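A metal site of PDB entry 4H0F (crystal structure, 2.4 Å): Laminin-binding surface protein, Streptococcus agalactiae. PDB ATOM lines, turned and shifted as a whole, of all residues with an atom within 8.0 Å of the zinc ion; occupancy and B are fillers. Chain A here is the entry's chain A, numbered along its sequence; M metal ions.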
ATOM      1  N   PHE A   8      -3.642 -14.835  13.545  1.00  0.00           N
ATOM      2  CA  PHE A   8      -4.664 -13.783  13.428  1.00  0.00           C
ATOM      3  C   PHE A   8      -4.303 -12.591  14.326  1.00  0.00           C
ATOM      4  O   PHE A   8      -3.338 -12.655  15.087  1.00  0.00           O
ATOM      5  CB  PHE A   8      -6.103 -14.353  13.662  1.00  0.00           C
ATOM      6  CG  PHE A   8      -6.449 -14.688  15.097  1.00  0.00           C
ATOM      7  CD1 PHE A   8      -5.716 -15.626  15.823  1.00  0.00           C
ATOM      8  CD2 PHE A   8      -7.561 -14.100  15.702  1.00  0.00           C
ATOM      9  CE1 PHE A   8      -6.087 -15.984  17.151  1.00  0.00           C
ATOM     10  CE2 PHE A   8      -7.946 -14.444  17.033  1.00  0.00           C
ATOM     11  CZ  PHE A   8      -7.206 -15.388  17.747  1.00  0.00           C
ATOM     12  N   ILE A  34     -11.932 -16.567  12.060  1.00  0.00           N
ATOM     13  CA  ILE A  34     -10.793 -17.344  12.520  1.00  0.00           C
ATOM     14  C   ILE A  34     -11.250 -18.709  13.024  1.00  0.00           C
ATOM     15  O   ILE A  34     -10.555 -19.696  12.862  1.00  0.00           O
ATOM     16  CB  ILE A  34     -10.033 -16.652  13.653  1.00  0.00           C
ATOM     17  CG1 ILE A  34      -8.785 -17.456  14.018  1.00  0.00           C
ATOM     18  CG2 ILE A  34     -10.919 -16.556  14.888  1.00  0.00           C
ATOM     19  CD1 ILE A  34      -7.853 -17.724  12.862  1.00  0.00           C
ATOM     20  N   HIS A  35     -12.440 -18.742  13.615  1.00  0.00           N
ATOM     21  CA  HIS A  35     -12.980 -19.997  14.160  1.00  0.00           C
ATOM     22  C   HIS A  35     -13.192 -21.060  13.117  1.00  0.00           C
ATOM     23  O   HIS A  35     -13.076 -22.250  13.392  1.00  0.00           O
ATOM     24  CB  HIS A  35     -14.296 -19.744  14.887  1.00  0.00           C
ATOM     25  CG  HIS A  35     -14.111 -19.155  16.242  1.00  0.00           C
ATOM     26  ND1 HIS A  35     -13.536 -19.860  17.286  1.00  0.00           N
ATOM     27  CD2 HIS A  35     -14.363 -17.919  16.728  1.00  0.00           C
ATOM     28  CE1 HIS A  35     -13.427 -19.075  18.332  1.00  0.00           C
ATOM     29  NE2 HIS A  35     -13.925 -17.894  18.027  1.00  0.00           N
ATOM     30  N   LEU A  60      -8.120 -23.799  18.876  1.00  0.00           N
ATOM     31  CA  LEU A  60      -8.708 -22.803  17.961  1.00  0.00           C
ATOM     32  C   LEU A  60      -8.229 -23.070  16.530  1.00  0.00           C
ATOM     33  O   LEU A  60      -9.015 -23.418  15.660  1.00  0.00           O
ATOM     34  CB  LEU A  60      -8.307 -21.379  18.386  1.00  0.00           C
ATOM     35  CG  LEU A  60      -8.798 -20.188  17.563  1.00  0.00           C
ATOM     36  CD1 LEU A  60     -10.294 -20.017  17.719  1.00  0.00           C
ATOM     37  CD2 LEU A  60      -8.066 -18.917  18.025  1.00  0.00           C
ATOM     38  N   ASP A  98     -12.300 -23.477  25.963  1.00  0.00           N
ATOM     39  CA  ASP A  98     -12.532 -22.103  25.539  1.00  0.00           C
ATOM     40  C   ASP A  98     -11.165 -21.487  25.282  1.00  0.00           C
ATOM     41  O   ASP A  98     -10.343 -21.420  26.189  1.00  0.00           O
ATOM     42  CB  ASP A  98     -13.218 -21.318  26.650  1.00  0.00           C
ATOM     43  CG  ASP A  98     -13.675 -19.948  26.200  1.00  0.00           C
ATOM     44  OD1 ASP A  98     -13.223 -19.487  25.128  1.00  0.00           O
ATOM     45  OD2 ASP A  98     -14.494 -19.328  26.919  1.00  0.00           O
ATOM     46  N   PRO A  99     -10.914 -21.011  24.056  1.00  0.00           N
ATOM     47  CA  PRO A  99      -9.636 -20.413  23.691  1.00  0.00           C
ATOM     48  C   PRO A  99      -9.512 -18.900  23.833  1.00  0.00           C
ATOM     49  O   PRO A  99      -8.422 -18.349  23.669  1.00  0.00           O
ATOM     50  CB  PRO A  99      -9.468 -20.870  22.247  1.00  0.00           C
ATOM     51  CG  PRO A  99     -10.847 -20.689  21.725  1.00  0.00           C
ATOM     52  CD  PRO A  99     -11.753 -21.193  22.850  1.00  0.00           C
ATOM     53  N   HIS A 100     -10.612 -18.218  24.150  1.00  0.00           N
ATOM     54  CA  HIS A 100     -10.636 -16.743  24.270  1.00  0.00           C
ATOM     55  C   HIS A 100      -9.930 -16.172  25.490  1.00  0.00           C
ATOM     56  O   HIS A 100     -10.542 -15.411  26.262  1.00  0.00           O
ATOM     57  CB  HIS A 100     -12.075 -16.240  24.259  1.00  0.00           C
ATOM     58  CG  HIS A 100     -12.883 -16.775  23.127  1.00  0.00           C
ATOM     59  ND1 HIS A 100     -13.750 -17.836  23.254  1.00  0.00           N
ATOM     60  CD2 HIS A 100     -12.930 -16.416  21.820  1.00  0.00           C
ATOM     61  CE1 HIS A 100     -14.290 -18.115  22.086  1.00  0.00           C
ATOM     62  NE2 HIS A 100     -13.813 -17.258  21.206  1.00  0.00           N
ATOM     63  N   TRP A 102      -7.052 -14.262  25.328  1.00  0.00           N
ATOM     64  CA  TRP A 102      -6.406 -12.993  25.023  1.00  0.00           C
ATOM     65  C   TRP A 102      -7.215 -11.793  25.471  1.00  0.00           C
ATOM     66  O   TRP A 102      -6.628 -10.765  25.820  1.00  0.00           O
ATOM     67  CB  TRP A 102      -6.050 -12.906  23.528  1.00  0.00           C
ATOM     68  CG  TRP A 102      -7.203 -13.000  22.578  1.00  0.00           C
ATOM     69  CD1 TRP A 102      -8.018 -11.968  22.166  1.00  0.00           C
ATOM     70  CD2 TRP A 102      -7.728 -14.188  21.994  1.00  0.00           C
ATOM     71  NE1 TRP A 102      -9.028 -12.454  21.365  1.00  0.00           N
ATOM     72  CE2 TRP A 102      -8.874 -13.817  21.249  1.00  0.00           C
ATOM     73  CE3 TRP A 102      -7.359 -15.537  22.028  1.00  0.00           C
ATOM     74  CZ2 TRP A 102      -9.666 -14.754  20.546  1.00  0.00           C
ATOM     75  CZ3 TRP A 102      -8.137 -16.473  21.326  1.00  0.00           C
ATOM     76  CH2 TRP A 102      -9.277 -16.069  20.598  1.00  0.00           C
ATOM     77  N   THR A 103      -8.536 -11.887  25.506  1.00  0.00           N
ATOM     78  CA  THR A 103      -9.336 -10.735  25.944  1.00  0.00           C
ATOM     79  C   THR A 103      -9.179 -10.502  27.452  1.00  0.00           C
ATOM     80  O   THR A 103      -9.749  -9.548  27.988  1.00  0.00           O
ATOM     81  CB  THR A 103     -10.872 -10.882  25.628  1.00  0.00           C
ATOM     82  OG1 THR A 103     -11.449 -11.914  26.461  1.00  0.00           O
ATOM     83  CG2 THR A 103     -11.091 -11.203  24.152  1.00  0.00           C
ATOM     84  N   HIS A 164     -21.127 -13.892  20.646  1.00  0.00           N
ATOM     85  CA  HIS A 164     -20.690 -15.286  20.846  1.00  0.00           C
ATOM     86  C   HIS A 164     -19.837 -15.384  22.119  1.00  0.00           C
ATOM     87  O   HIS A 164     -19.361 -14.372  22.637  1.00  0.00           O
ATOM     88  CB  HIS A 164     -20.013 -15.888  19.577  1.00  0.00           C
ATOM     89  CG  HIS A 164     -18.561 -15.568  19.406  1.00  0.00           C
ATOM     90  ND1 HIS A 164     -18.112 -14.369  18.869  1.00  0.00           N
ATOM     91  CD2 HIS A 164     -17.452 -16.329  19.603  1.00  0.00           C
ATOM     92  CE1 HIS A 164     -16.798 -14.416  18.743  1.00  0.00           C
ATOM     93  NE2 HIS A 164     -16.374 -15.596  19.170  1.00  0.00           N
ATOM     94  N   THR A 165     -19.678 -16.578  22.679  1.00  0.00           N
ATOM     95  CA  THR A 165     -18.936 -16.717  23.921  1.00  0.00           C
ATOM     96  C   THR A 165     -17.434 -16.439  23.794  1.00  0.00           C
ATOM     97  O   THR A 165     -16.617 -17.359  23.749  1.00  0.00           O
ATOM     98  CB  THR A 165     -19.140 -18.120  24.515  1.00  0.00           C
ATOM     99  OG1 THR A 165     -20.510 -18.500  24.349  1.00  0.00           O
ATOM    100  CG2 THR A 165     -18.782 -18.155  25.994  1.00  0.00           C
ATOM    101  N   ALA A 166     -17.065 -15.165  23.770  1.00  0.00           N
ATOM    102  CA  ALA A 166     -15.658 -14.791  23.608  1.00  0.00           C
ATOM    103  C   ALA A 166     -15.101 -13.918  24.732  1.00  0.00           C
ATOM    104  O   ALA A 166     -13.996 -13.404  24.612  1.00  0.00           O
ATOM    105  CB  ALA A 166     -15.446 -14.099  22.272  1.00  0.00           C
ATOM    106  N   PHE A 167     -15.829 -13.758  25.820  1.00  0.00           N
ATOM    107  CA  PHE A 167     -15.312 -12.934  26.892  1.00  0.00           C
ATOM    108  C   PHE A 167     -15.391 -13.608  28.276  1.00  0.00           C
ATOM    109  O   PHE A 167     -15.349 -12.941  29.317  1.00  0.00           O
ATOM    110  CB  PHE A 167     -16.043 -11.582  26.882  1.00  0.00           C
ATOM    111  CG  PHE A 167     -16.098 -10.936  25.510  1.00  0.00           C
ATOM    112  CD1 PHE A 167     -17.102 -11.278  24.605  1.00  0.00           C
ATOM    113  CD2 PHE A 167     -15.111 -10.039  25.107  1.00  0.00           C
ATOM    114  CE1 PHE A 167     -17.128 -10.733  23.306  1.00  0.00           C
ATOM    115  CE2 PHE A 167     -15.123  -9.495  23.818  1.00  0.00           C
ATOM    116  CZ  PHE A 167     -16.127  -9.837  22.914  1.00  0.00           C
ATOM    117  N   GLY A 183     -22.199 -19.983  20.592  1.00  0.00           N
ATOM    118  CA  GLY A 183     -21.178 -20.674  21.363  1.00  0.00           C
ATOM    119  C   GLY A 183     -19.767 -20.166  21.146  1.00  0.00           C
ATOM    120  O   GLY A 183     -19.578 -19.039  20.671  1.00  0.00           O
ATOM    121  N   ILE A 184     -18.780 -20.987  21.513  1.00  0.00           N
ATOM    122  CA  ILE A 184     -17.372 -20.630  21.368  1.00  0.00           C
ATOM    123  C   ILE A 184     -17.068 -20.110  19.969  1.00  0.00           C
ATOM    124  O   ILE A 184     -16.095 -19.379  19.747  1.00  0.00           O
ATOM    125  CB  ILE A 184     -16.456 -21.850  21.694  1.00  0.00           C
ATOM    126  CG1 ILE A 184     -16.357 -22.023  23.202  1.00  0.00           C
ATOM    127  CG2 ILE A 184     -15.067 -21.665  21.137  1.00  0.00           C
ATOM    128  CD1 ILE A 184     -17.648 -22.424  23.809  1.00  0.00           C
ATOM    129  N   SER A 185     -17.908 -20.485  19.009  1.00  0.00           N
ATOM    130  CA  SER A 185     -17.723 -20.013  17.649  1.00  0.00           C
ATOM    131  C   SER A 185     -19.041 -19.391  17.205  1.00  0.00           C
ATOM    132  O   SER A 185     -20.106 -19.850  17.602  1.00  0.00           O
ATOM    133  CB  SER A 185     -17.364 -21.159  16.734  1.00  0.00           C
ATOM    134  OG  SER A 185     -17.293 -20.711  15.397  1.00  0.00           O
ATOM    135  N   PRO A 186     -18.976 -18.338  16.387  1.00  0.00           N
ATOM    136  CA  PRO A 186     -20.181 -17.657  15.886  1.00  0.00           C
ATOM    137  C   PRO A 186     -21.085 -18.505  15.005  1.00  0.00           C
ATOM    138  O   PRO A 186     -22.266 -18.192  14.869  1.00  0.00           O
ATOM    139  CB  PRO A 186     -19.598 -16.467  15.125  1.00  0.00           C
ATOM    140  CG  PRO A 186     -18.347 -16.171  15.873  1.00  0.00           C
ATOM    141  CD  PRO A 186     -17.769 -17.558  16.067  1.00  0.00           C
ATOM    142  N   GLU A 213     -21.147  -7.828  17.388  1.00  0.00           N
ATOM    143  CA  GLU A 213     -19.788  -7.645  16.912  1.00  0.00           C
ATOM    144  C   GLU A 213     -19.783  -7.404  15.409  1.00  0.00           C
ATOM    145  O   GLU A 213     -20.677  -7.853  14.700  1.00  0.00           O
ATOM    146  CB  GLU A 213     -18.902  -8.846  17.282  1.00  0.00           C
ATOM    147  CG  GLU A 213     -19.266 -10.158  16.625  1.00  0.00           C
ATOM    148  CD  GLU A 213     -18.371 -11.281  17.113  1.00  0.00           C
ATOM    149  OE1 GLU A 213     -17.156 -11.218  16.845  1.00  0.00           O
ATOM    150  OE2 GLU A 213     -18.882 -12.209  17.764  1.00  0.00           O
ATOM    151  N   ASN A 215     -18.102  -8.669  13.132  1.00  0.00           N
ATOM    152  CA  ASN A 215     -17.906  -9.899  12.350  1.00  0.00           C
ATOM    153  C   ASN A 215     -19.179 -10.648  11.919  1.00  0.00           C
ATOM    154  O   ASN A 215     -19.178 -11.315  10.879  1.00  0.00           O
ATOM    155  CB  ASN A 215     -17.004 -10.857  13.136  1.00  0.00           C
ATOM    156  CG  ASN A 215     -15.693 -10.204  13.589  1.00  0.00           C
ATOM    157  OD1 ASN A 215     -14.915  -9.717  12.774  1.00  0.00           O
ATOM    158  ND2 ASN A 215     -15.467 -10.192  14.912  1.00  0.00           N
ATOM    159  N   PRO A 237     -14.249  -8.951  20.161  1.00  0.00           N
ATOM    160  CA  PRO A 237     -13.479 -10.052  20.763  1.00  0.00           C
ATOM    161  C   PRO A 237     -12.027 -10.072  20.238  1.00  0.00           C
ATOM    162  O   PRO A 237     -11.221 -10.967  20.576  1.00  0.00           O
ATOM    163  CB  PRO A 237     -14.269 -11.306  20.354  1.00  0.00           C
ATOM    164  CG  PRO A 237     -14.833 -10.896  19.017  1.00  0.00           C
ATOM    165  CD  PRO A 237     -15.305  -9.473  19.281  1.00  0.00           C
ATOM    166  N   LEU A 238     -11.734  -9.056  19.427  1.00  0.00           N
ATOM    167  CA  LEU A 238     -10.430  -8.832  18.805  1.00  0.00           C
ATOM    168  C   LEU A 238      -9.986  -9.967  17.925  1.00  0.00           C
ATOM    169  O   LEU A 238      -8.785 -10.212  17.788  1.00  0.00           O
ATOM    170  CB  LEU A 238      -9.356  -8.544  19.853  1.00  0.00           C
ATOM    171  CG  LEU A 238      -9.505  -7.213  20.605  1.00  0.00           C
ATOM    172  CD1 LEU A 238      -8.392  -7.042  21.631  1.00  0.00           C
ATOM    173  CD2 LEU A 238      -9.473  -6.074  19.599  1.00  0.00           C
ATOM    174  N   GLU A 239     -10.938 -10.666  17.337  1.00  0.00           N
ATOM    175  CA  GLU A 239     -10.595 -11.779  16.470  1.00  0.00           C
ATOM    176  C   GLU A 239     -10.321 -11.222  15.097  1.00  0.00           C
ATOM    177  O   GLU A 239      -9.704 -11.861  14.258  1.00  0.00           O
ATOM    178  CB  GLU A 239     -11.729 -12.794  16.458  1.00  0.00           C
ATOM    179  CG  GLU A 239     -12.167 -13.103  17.856  1.00  0.00           C
ATOM    180  CD  GLU A 239     -13.007 -14.337  17.950  1.00  0.00           C
ATOM    181  OE1 GLU A 239     -13.735 -14.618  16.971  1.00  0.00           O
ATOM    182  OE2 GLU A 239     -12.936 -14.986  19.015  1.00  0.00           O
HETATM  183 ZN    ZN M   1     -14.288 -16.441  19.217  1.00  0.00          ZN
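NE2 of His 35 sits close to O of Ile 184 (3.1 Å). A ring nitrogen (NE2) of His 100 lies close to the backbone carbonyl oxygen of Ile 184 (3.4 Å). A ring nitrogen (ND1) of His 100 is in hydrogen-bond range of the backbone carbonyl oxygen of Thr 165 (2.9 Å). A ring nitrogen (ND1) of His 100 sits at hydrogen-bond distance from the side-chain carboxylate (OD1) of Asp 98 (2.6 Å). ND1 of His 164 lies within hydrogen-bond range of OE2 of Glu 213 (2.5 Å).
Merely in contact with the zinc ion: Ile 184. Of the 22 residues printed, 5 come within 4 Å of the zinc ion. The nearest printed residue that does not touch the zinc ion is Ala 166 (4.02 Å).
The zinc ion is bound by a ring nitrogen (NE2) of His 35 (1.9 Å), the side-chain carboxylate (OE2) of Glu 239 (2.0 Å), a ring nitrogen (NE2) of His 100 (2.2 Å) and a ring nitrogen (NE2) of His 164 (2.3 Å). The zinc ion has four donor atoms within binding distance.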
